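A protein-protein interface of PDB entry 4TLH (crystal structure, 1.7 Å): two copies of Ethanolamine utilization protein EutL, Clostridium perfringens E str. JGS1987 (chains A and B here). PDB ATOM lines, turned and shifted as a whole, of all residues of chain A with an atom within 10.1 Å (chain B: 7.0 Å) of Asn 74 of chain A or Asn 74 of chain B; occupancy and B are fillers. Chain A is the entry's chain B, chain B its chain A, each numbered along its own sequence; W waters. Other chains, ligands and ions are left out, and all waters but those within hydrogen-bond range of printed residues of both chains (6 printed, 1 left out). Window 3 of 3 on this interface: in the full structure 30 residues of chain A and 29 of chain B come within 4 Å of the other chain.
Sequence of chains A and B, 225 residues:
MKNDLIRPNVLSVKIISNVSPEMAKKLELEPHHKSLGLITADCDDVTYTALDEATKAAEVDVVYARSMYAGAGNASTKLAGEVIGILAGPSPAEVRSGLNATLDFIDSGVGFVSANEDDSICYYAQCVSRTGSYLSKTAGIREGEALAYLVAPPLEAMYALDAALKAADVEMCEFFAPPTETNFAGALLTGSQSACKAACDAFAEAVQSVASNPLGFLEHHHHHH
Of the 20 printed residues of chain A, 3 touch a printed residue of chain B. Hydrophobic or aromatic side chains of chain A within 4 Å of the printed part of chain B: Met 68 and Tyr 69. Hydrophobic or aromatic side chains of chain B within 4 Å of the printed part of chain A: Tyr 69 and Ala 70.
Tyr 69 of chain B touches its own counterpart, Tyr 69 of chain A. Tyr 69 of chain A touches Ala 70 of chain B, but with the chains exchanged Ala 70 of chain A does not touch Tyr 69 of chain B (6.1 Å). Tyr 69 of chain A touches Asn 183 of chain B, but with the chains exchanged Asn 183 of chain A does not touch Tyr 69 of chain B (8.2 Å). Asn 74 of chain A touches its own counterpart, Asn 74 of chain B. Positions printed for both chains: 69, 70, 71, 72, 73, 74, 75, 76, 77, 81 and 183. Of the 5 pairs that touch across the chains among the printed residues, 2 have their exchanged pair printed and touching as well.
Asn 74 of chain A touches one residue of chain B. Printed residues of chain A within 4 Å of Tyr 69 of chain B: Tyr 69 (3.9 Å). No residue of chain A comes within 4 Å of Gly 71 of chain B. No residue of chain A comes within 4 Å of Ala 72 of chain B. Printed residues of chain A within 4 Å of Asn 74 of chain B: Asn 74. No residue of chain A comes within 4 Å of Ala 75 of chain B. Thr 77 of chain B touches none of the printed residues of chain A. Of the printed residues of chain A, Asn 183 of chain B touches Met 68 and Tyr 69. The nearest residue of chain B that does not touch Asn 74 of chain A is Ala 70 of chain B (4.6 Å).
The backbone carbonyl oxygen of Ala 70 of chain B is in hydrogen-bond range of the side-chain amide nitrogen of Asn 74 of chain B, at 2.8 Å. The backbone NH of Met 68 of chain A sits at hydrogen-bond distance from the backbone carbonyl oxygen of Glu 82 of chain A (3.0 Å). ND2 of Asn 74 of chain A sits at hydrogen-bond distance from O of Ala 70 of chain A (2.8 Å).
Among the printed residues, pairs that only touch across the chains: Met 68 of chain A with Asn 183 of chain B (3.6 Å), Tyr 69 of chain A with Tyr 69 of chain B (3.9 Å) and Tyr 69 of chain A with Ala 70 of chain B (3.99 Å).
The side-chain amide nitrogen (ND2) of Asn 74 of chain B lies within hydrogen-bond range of the backbone carbonyl oxygen (O) of Asn 74 of chain A. The backbone NH (N) of Tyr 69 of chain A is in hydrogen-bond range of the side-chain amide oxygen (OD1) of Asn 183 of chain B (2.9 Å).
Water W5 lies within hydrogen-bond range of the side-chain hydroxyl (OG) of Ser 76 of chain A (2.7 Å) and the backbone carbonyl oxygen (O) of Ala 70 of chain B (3.4 Å). Water W2 lies within hydrogen-bond range of the backbone carbonyl oxygen of Tyr 69 of chain A (2.7 Å), the backbone carbonyl oxygen of Gly 71 of chain A (2.7 Å), the side-chain amide nitrogen of Asn 183 of chain B (3.1 Å) and the backbone NH of Ala 75 of chain A (3.5 Å). Water W4 lies within hydrogen-bond range of the backbone carbonyl oxygen of Asn 183 of chain B and the side-chain hydroxyl of Thr 77 of chain A. Water W1 lies within hydrogen-bond range of ND2 of Asn 183 of chain B (3.0 Å), O of Asn 74 of chain A (3.1 Å) and O of Ala 70 of chain B (3.3 Å). Water W6 bridges the side-chain amide oxygen of Asn 74 of chain A (3.3 Å) and the side-chain amide oxygen of Asn 74 of chain B (3.3 Å). Water W3 lies within hydrogen-bond range of OH of Tyr 69 of chain B (3.3 Å) and OH of Tyr 69 of chain A (3.4 Å).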
ATOM      1  N   LEU A  11     -22.620  -3.563 -32.166  1.00  0.00           N
ATOM      2  CA  LEU A  11     -22.690  -2.115 -32.025  1.00  0.00           C
ATOM      3  C   LEU A  11     -21.350  -1.402 -32.193  1.00  0.00           C
ATOM      4  O   LEU A  11     -21.309  -0.267 -32.662  1.00  0.00           O
ATOM      5  CB  LEU A  11     -23.274  -1.770 -30.659  1.00  0.00           C
ATOM      6  CG  LEU A  11     -24.676  -2.352 -30.408  1.00  0.00           C
ATOM      7  CD1 LEU A  11     -25.145  -2.075 -28.977  1.00  0.00           C
ATOM      8  CD2 LEU A  11     -25.686  -1.803 -31.384  1.00  0.00           C
ATOM      9  N   ASP A  42     -25.973  -6.236 -28.992  1.00  0.00           N
ATOM     10  CA  ASP A  42     -27.262  -6.100 -28.309  1.00  0.00           C
ATOM     11  C   ASP A  42     -27.862  -7.439 -27.875  1.00  0.00           C
ATOM     12  O   ASP A  42     -29.038  -7.499 -27.521  1.00  0.00           O
ATOM     13  CB  ASP A  42     -28.262  -5.336 -29.193  1.00  0.00           C
ATOM     14  CG  ASP A  42     -28.656  -6.093 -30.460  1.00  0.00           C
ATOM     15  OD1 ASP A  42     -28.299  -7.285 -30.609  1.00  0.00           O
ATOM     16  OD2 ASP A  42     -29.346  -5.484 -31.313  1.00  0.00           O
ATOM     17  N   MET A  68     -24.824  -6.663 -19.467  1.00  0.00           N
ATOM     18  CA  MET A  68     -25.250  -5.407 -18.867  1.00  0.00           C
ATOM     19  C   MET A  68     -26.578  -5.529 -18.133  1.00  0.00           C
ATOM     20  O   MET A  68     -27.472  -6.228 -18.595  1.00  0.00           O
ATOM     21  CB  MET A  68     -25.399  -4.335 -19.939  1.00  0.00           C
ATOM     22  CG  MET A  68     -24.154  -4.127 -20.816  1.00  0.00           C
ATOM     23  SD  MET A  68     -22.798  -3.376 -19.901  1.00  0.00           S
ATOM     24  CE  MET A  68     -21.562  -4.649 -19.979  1.00  0.00           C
ATOM     25  N   TYR A  69     -26.713  -4.797 -17.034  1.00  0.00           N
ATOM     26  CA  TYR A  69     -27.936  -4.824 -16.248  1.00  0.00           C
ATOM     27  C   TYR A  69     -29.152  -4.339 -17.020  1.00  0.00           C
ATOM     28  O   TYR A  69     -29.155  -3.263 -17.592  1.00  0.00           O
ATOM     29  CB  TYR A  69     -27.789  -3.987 -14.975  1.00  0.00           C
ATOM     30  CG  TYR A  69     -26.752  -4.536 -14.032  1.00  0.00           C
ATOM     31  CD1 TYR A  69     -26.961  -5.711 -13.359  1.00  0.00           C
ATOM     32  CD2 TYR A  69     -25.550  -3.881 -13.839  1.00  0.00           C
ATOM     33  CE1 TYR A  69     -26.009  -6.223 -12.503  1.00  0.00           C
ATOM     34  CE2 TYR A  69     -24.591  -4.382 -12.985  1.00  0.00           C
ATOM     35  CZ  TYR A  69     -24.825  -5.561 -12.324  1.00  0.00           C
ATOM     36  OH  TYR A  69     -23.868  -6.068 -11.467  1.00  0.00           O
ATOM     37  N   ALA A  70     -30.176  -5.192 -17.020  1.00  0.00           N
ATOM     38  CA  ALA A  70     -31.499  -4.917 -17.580  1.00  0.00           C
ATOM     39  C   ALA A  70     -31.566  -4.972 -19.114  1.00  0.00           C
ATOM     40  O   ALA A  70     -32.577  -4.603 -19.715  1.00  0.00           O
ATOM     41  CB  ALA A  70     -32.006  -3.568 -17.065  1.00  0.00           C
ATOM     42  N   GLY A  71     -30.512  -5.457 -19.751  1.00  0.00           N
ATOM     43  CA  GLY A  71     -30.578  -5.762 -21.177  1.00  0.00           C
ATOM     44  C   GLY A  71     -30.468  -4.598 -22.142  1.00  0.00           C
ATOM     45  O   GLY A  71     -30.466  -3.436 -21.742  1.00  0.00           O
ATOM     46  N   ALA A  72     -30.420  -4.915 -23.433  1.00  0.00           N
ATOM     47  CA  ALA A  72     -30.096  -3.930 -24.456  1.00  0.00           C
ATOM     48  C   ALA A  72     -31.179  -2.891 -24.610  1.00  0.00           C
ATOM     49  O   ALA A  72     -30.889  -1.735 -24.908  1.00  0.00           O
ATOM     50  CB  ALA A  72     -29.850  -4.626 -25.802  1.00  0.00           C
ATOM     51  N   GLY A  73     -32.424  -3.307 -24.416  1.00  0.00           N
ATOM     52  CA  GLY A  73     -33.564  -2.421 -24.521  1.00  0.00           C
ATOM     53  C   GLY A  73     -33.526  -1.298 -23.503  1.00  0.00           C
ATOM     54  O   GLY A  73     -34.170  -0.262 -23.694  1.00  0.00           O
ATOM     55  N   ASN A  74     -32.756  -1.497 -22.438  1.00  0.00           N
ATOM     56  CA  ASN A  74     -32.618  -0.490 -21.389  1.00  0.00           C
ATOM     57  C   ASN A  74     -31.245   0.177 -21.353  1.00  0.00           C
ATOM     58  O   ASN A  74     -30.943   0.931 -20.415  1.00  0.00           O
ATOM     59  CB  ASN A  74     -32.922  -1.113 -20.029  1.00  0.00           C
ATOM     60  CG  ASN A  74     -34.404  -1.485 -19.879  1.00  0.00           C
ATOM     61  OD1 ASN A  74     -35.284  -0.656 -20.115  1.00  0.00           O
ATOM     62  ND2 ASN A  74     -34.675  -2.736 -19.531  1.00  0.00           N
ATOM     63  N   ALA A  75     -30.423  -0.046 -22.384  1.00  0.00           N
ATOM     64  CA  ALA A  75     -29.144   0.665 -22.469  1.00  0.00           C
ATOM     65  C   ALA A  75     -29.350   2.173 -22.472  1.00  0.00           C
ATOM     66  O   ALA A  75     -30.290   2.682 -23.086  1.00  0.00           O
ATOM     67  CB  ALA A  75     -28.369   0.250 -23.718  1.00  0.00           C
ATOM     68  N   SER A  76     -28.453   2.893 -21.794  1.00  0.00           N
ATOM     69  CA  SER A  76     -28.556   4.340 -21.706  1.00  0.00           C
ATOM     70  C   SER A  76     -27.612   5.036 -22.669  1.00  0.00           C
ATOM     71  O   SER A  76     -27.734   6.233 -22.882  1.00  0.00           O
ATOM     72  CB  SER A  76     -28.258   4.827 -20.290  1.00  0.00           C
ATOM     73  OG  SER A  76     -26.907   4.596 -19.952  1.00  0.00           O
ATOM     74  N   THR A  77     -26.680   4.278 -23.227  1.00  0.00           N
ATOM     75  CA  THR A  77     -25.762   4.787 -24.220  1.00  0.00           C
ATOM     76  C   THR A  77     -25.737   3.896 -25.463  1.00  0.00           C
ATOM     77  O   THR A  77     -26.191   2.757 -25.451  1.00  0.00           O
ATOM     78  CB  THR A  77     -24.340   4.921 -23.659  1.00  0.00           C
ATOM     79  OG1 THR A  77     -23.823   3.631 -23.340  1.00  0.00           O
ATOM     80  CG2 THR A  77     -24.324   5.805 -22.410  1.00  0.00           C
ATOM     81  N   LYS A  78     -25.176   4.456 -26.529  1.00  0.00           N
ATOM     82  CA  LYS A  78     -25.301   3.917 -27.875  1.00  0.00           C
ATOM     83  C   LYS A  78     -24.595   2.584 -28.058  1.00  0.00           C
ATOM     84  O   LYS A  78     -25.128   1.691 -28.730  1.00  0.00           O
ATOM     85  CB  LYS A  78     -24.741   4.945 -28.869  1.00  0.00           C
ATOM     86  CG  LYS A  78     -24.945   4.606 -30.331  1.00  0.00           C
ATOM     87  CD  LYS A  78     -24.217   5.623 -31.210  1.00  0.00           C
ATOM     88  CE  LYS A  78     -24.428   5.336 -32.684  1.00  0.00           C
ATOM     89  NZ  LYS A  78     -25.883   5.278 -33.023  1.00  0.00           N
ATOM     90  N   ALA A  80     -23.308   0.498 -25.505  1.00  0.00           N
ATOM     91  CA  ALA A  80     -23.293  -0.433 -24.393  1.00  0.00           C
ATOM     92  C   ALA A  80     -23.973  -1.759 -24.726  1.00  0.00           C
ATOM     93  O   ALA A  80     -23.506  -2.826 -24.306  1.00  0.00           O
ATOM     94  CB  ALA A  80     -23.951   0.202 -23.201  1.00  0.00           C
ATOM     95  N   GLY A  81     -25.101  -1.695 -25.428  1.00  0.00           N
ATOM     96  CA  GLY A  81     -25.890  -2.885 -25.719  1.00  0.00           C
ATOM     97  C   GLY A  81     -26.181  -3.669 -24.460  1.00  0.00           C
ATOM     98  O   GLY A  81     -26.627  -3.104 -23.429  1.00  0.00           O
ATOM     99  N   GLU A  82     -25.933  -4.971 -24.519  1.00  0.00           N
ATOM    100  CA  GLU A  82     -26.001  -5.775 -23.311  1.00  0.00           C
ATOM    101  C   GLU A  82     -24.831  -6.713 -23.132  1.00  0.00           C
ATOM    102  O   GLU A  82     -24.887  -7.613 -22.312  1.00  0.00           O
ATOM    103  CB  GLU A  82     -27.302  -6.564 -23.266  1.00  0.00           C
ATOM    104  CG  GLU A  82     -27.492  -7.600 -24.341  1.00  0.00           C
ATOM    105  CD  GLU A  82     -28.809  -8.375 -24.163  1.00  0.00           C
ATOM    106  OE1 GLU A  82     -29.846  -7.747 -23.807  1.00  0.00           O
ATOM    107  OE2 GLU A  82     -28.810  -9.613 -24.390  1.00  0.00           O
ATOM    108  N   GLU A 181     -27.637 -10.653 -15.376  1.00  0.00           N
ATOM    109  CA  GLU A 181     -27.711  -9.186 -15.487  1.00  0.00           C
ATOM    110  C   GLU A 181     -28.889  -8.770 -16.384  1.00  0.00           C
ATOM    111  O   GLU A 181     -29.566  -7.765 -16.125  1.00  0.00           O
ATOM    112  CB  GLU A 181     -26.397  -8.599 -16.039  1.00  0.00           C
ATOM    113  CG  GLU A 181     -25.253  -8.619 -15.059  1.00  0.00           C
ATOM    114  CD  GLU A 181     -24.459  -9.915 -15.042  1.00  0.00           C
ATOM    115  OE1 GLU A 181     -24.755 -10.850 -15.819  1.00  0.00           O
ATOM    116  OE2 GLU A 181     -23.508  -9.981 -14.227  1.00  0.00           O
ATOM    117  N   THR A 182     -29.163  -9.559 -17.412  1.00  0.00           N
ATOM    118  CA  THR A 182     -30.246  -9.237 -18.357  1.00  0.00           C
ATOM    119  C   THR A 182     -31.617  -9.767 -17.914  1.00  0.00           C
ATOM    120  O   THR A 182     -32.585  -9.680 -18.663  1.00  0.00           O
ATOM    121  CB  THR A 182     -29.947  -9.801 -19.751  1.00  0.00           C
ATOM    122  OG1 THR A 182     -29.784 -11.224 -19.681  1.00  0.00           O
ATOM    123  CG2 THR A 182     -28.670  -9.160 -20.328  1.00  0.00           C
ATOM    124  N   ASN A 183     -31.684 -10.321 -16.709  1.00  0.00           N
ATOM    125  CA  ASN A 183     -32.951 -10.849 -16.151  1.00  0.00           C
ATOM    126  C   ASN A 183     -33.457 -12.067 -16.917  1.00  0.00           C
ATOM    127  O   ASN A 183     -34.679 -12.296 -17.053  1.00  0.00           O
ATOM    128  CB  ASN A 183     -34.025  -9.759 -16.102  1.00  0.00           C
ATOM    129  CG  ASN A 183     -33.643  -8.623 -15.170  1.00  0.00           C
ATOM    130  OD1 ASN A 183     -33.125  -8.857 -14.073  1.00  0.00           O
ATOM    131  ND2 ASN A 183     -33.881  -7.382 -15.605  1.00  0.00           N
ATOM    132  N   PHE A 184     -32.502 -12.862 -17.394  1.00  0.00           N
ATOM    133  CA  PHE A 184     -32.788 -14.190 -17.911  1.00  0.00           C
ATOM    134  C   PHE A 184     -32.205 -15.239 -16.961  1.00  0.00           C
ATOM    135  O   PHE A 184     -31.737 -14.926 -15.850  1.00  0.00           O
ATOM    136  CB  PHE A 184     -32.228 -14.351 -19.342  1.00  0.00           C
ATOM    137  CG  PHE A 184     -33.063 -13.667 -20.401  1.00  0.00           C
ATOM    138  CD1 PHE A 184     -33.115 -12.286 -20.473  1.00  0.00           C
ATOM    139  CD2 PHE A 184     -33.774 -14.410 -21.339  1.00  0.00           C
ATOM    140  CE1 PHE A 184     -33.874 -11.646 -21.443  1.00  0.00           C
ATOM    141  CE2 PHE A 184     -34.537 -13.784 -22.311  1.00  0.00           C
ATOM    142  CZ  PHE A 184     -34.597 -12.398 -22.366  1.00  0.00           C
ATOM    143  N   TYR B  69     -29.165   0.347 -10.307  1.00  0.00           N
ATOM    144  CA  TYR B  69     -29.058  -0.531 -11.472  1.00  0.00           C
ATOM    145  C   TYR B  69     -29.700   0.076 -12.707  1.00  0.00           C
ATOM    146  O   TYR B  69     -30.868   0.460 -12.679  1.00  0.00           O
ATOM    147  CB  TYR B  69     -29.685  -1.889 -11.183  1.00  0.00           C
ATOM    148  CG  TYR B  69     -28.937  -2.679 -10.144  1.00  0.00           C
ATOM    149  CD1 TYR B  69     -27.726  -3.284 -10.434  1.00  0.00           C
ATOM    150  CD2 TYR B  69     -29.438  -2.807  -8.865  1.00  0.00           C
ATOM    151  CE1 TYR B  69     -27.049  -4.014  -9.469  1.00  0.00           C
ATOM    152  CE2 TYR B  69     -28.781  -3.527  -7.906  1.00  0.00           C
ATOM    153  CZ  TYR B  69     -27.584  -4.122  -8.203  1.00  0.00           C
ATOM    154  OH  TYR B  69     -26.933  -4.841  -7.229  1.00  0.00           O
ATOM    155  N   ALA B  70     -28.901   0.156 -13.775  1.00  0.00           N
ATOM    156  CA  ALA B  70     -29.322   0.598 -15.116  1.00  0.00           C
ATOM    157  C   ALA B  70     -29.521   2.105 -15.233  1.00  0.00           C
ATOM    158  O   ALA B  70     -30.047   2.588 -16.233  1.00  0.00           O
ATOM    159  CB  ALA B  70     -30.593  -0.140 -15.560  1.00  0.00           C
ATOM    160  N   GLY B  71     -29.114   2.861 -14.217  1.00  0.00           N
ATOM    161  CA  GLY B  71     -28.988   4.302 -14.364  1.00  0.00           C
ATOM    162  C   GLY B  71     -30.268   5.116 -14.209  1.00  0.00           C
ATOM    163  O   GLY B  71     -31.387   4.568 -14.155  1.00  0.00           O
ATOM    164  N   ALA B  72     -30.085   6.442 -14.160  1.00  0.00           N
ATOM    165  CA  ALA B  72     -31.156   7.392 -13.849  1.00  0.00           C
ATOM    166  C   ALA B  72     -32.273   7.357 -14.871  1.00  0.00           C
ATOM    167  O   ALA B  72     -33.440   7.554 -14.531  1.00  0.00           O
ATOM    168  CB  ALA B  72     -30.593   8.807 -13.757  1.00  0.00           C
ATOM    169  N   GLY B  73     -31.912   7.100 -16.123  1.00  0.00           N
ATOM    170  CA  GLY B  73     -32.873   7.059 -17.215  1.00  0.00           C
ATOM    171  C   GLY B  73     -33.872   5.923 -17.057  1.00  0.00           C
ATOM    172  O   GLY B  73     -34.979   5.988 -17.583  1.00  0.00           O
ATOM    173  N   ASN B  74     -33.480   4.898 -16.307  1.00  0.00           N
ATOM    174  CA  ASN B  74     -34.345   3.758 -16.000  1.00  0.00           C
ATOM    175  C   ASN B  74     -34.905   3.720 -14.584  1.00  0.00           C
ATOM    176  O   ASN B  74     -35.504   2.701 -14.166  1.00  0.00           O
ATOM    177  CB  ASN B  74     -33.561   2.478 -16.268  1.00  0.00           C
ATOM    178  CG  ASN B  74     -33.336   2.263 -17.739  1.00  0.00           C
ATOM    179  OD1 ASN B  74     -34.268   2.383 -18.523  1.00  0.00           O
ATOM    180  ND2 ASN B  74     -32.086   2.005 -18.133  1.00  0.00           N
ATOM    181  N   ALA B  75     -34.751   4.815 -13.840  1.00  0.00           N
ATOM    182  CA  ALA B  75     -35.342   4.879 -12.506  1.00  0.00           C
ATOM    183  C   ALA B  75     -36.860   4.728 -12.600  1.00  0.00           C
ATOM    184  O   ALA B  75     -37.495   5.239 -13.513  1.00  0.00           O
ATOM    185  CB  ALA B  75     -34.983   6.166 -11.825  1.00  0.00           C
ATOM    186  N   SER B  76     -37.446   4.026 -11.646  1.00  0.00           N
ATOM    187  CA  SER B  76     -38.871   3.744 -11.677  1.00  0.00           C
ATOM    188  C   SER B  76     -39.618   4.707 -10.767  1.00  0.00           C
ATOM    189  O   SER B  76     -40.846   4.788 -10.821  1.00  0.00           O
ATOM    190  CB  SER B  76     -39.126   2.307 -11.248  1.00  0.00           C
ATOM    191  OG  SER B  76     -38.662   2.127  -9.919  1.00  0.00           O
ATOM    192  N   THR B  77     -38.868   5.410  -9.911  1.00  0.00           N
ATOM    193  CA  THR B  77     -39.460   6.383  -9.003  1.00  0.00           C
ATOM    194  C   THR B  77     -38.735   7.719  -9.135  1.00  0.00           C
ATOM    195  O   THR B  77     -37.644   7.801  -9.670  1.00  0.00           O
ATOM    196  CB  THR B  77     -39.437   5.917  -7.509  1.00  0.00           C
ATOM    197  OG1 THR B  77     -38.090   5.741  -7.066  1.00  0.00           O
ATOM    198  CG2 THR B  77     -40.207   4.603  -7.330  1.00  0.00           C
ATOM    199  N   GLY B  81     -33.055   8.406  -8.867  1.00  0.00           N
ATOM    200  CA  GLY B  81     -31.926   8.838  -9.678  1.00  0.00           C
ATOM    201  C   GLY B  81     -31.017   7.673  -9.992  1.00  0.00           C
ATOM    202  O   GLY B  81     -31.501   6.575 -10.302  1.00  0.00           O
ATOM    203  N   ASN B 183     -24.019   0.525 -15.792  1.00  0.00           N
ATOM    204  CA  ASN B 183     -23.549  -0.049 -17.072  1.00  0.00           C
ATOM    205  C   ASN B 183     -22.493   0.820 -17.737  1.00  0.00           C
ATOM    206  O   ASN B 183     -22.432   0.958 -18.966  1.00  0.00           O
ATOM    207  CB  ASN B 183     -24.718  -0.301 -18.019  1.00  0.00           C
ATOM    208  CG  ASN B 183     -25.626  -1.400 -17.504  1.00  0.00           C
ATOM    209  OD1 ASN B 183     -25.151  -2.374 -16.921  1.00  0.00           O
ATOM    210  ND2 ASN B 183     -26.925  -1.233 -17.677  1.00  0.00           N
HETATM  211  O   HOH W   1     -28.378   1.163 -18.717  1.00  0.00           O
HETATM  212  O   HOH W   2     -28.897  -2.031 -19.985  1.00  0.00           O
HETATM  213  O   HOH W   3     -25.024  -7.274  -8.466  1.00  0.00           O
HETATM  214  O   HOH W   4     -23.869   2.686 -20.510  1.00  0.00           O
HETATM  215  O   HOH W   5     -27.103   3.931 -17.381  1.00  0.00           O
HETATM  216  O   HOH W   6     -35.761   2.262 -21.504  1.00  0.00           O
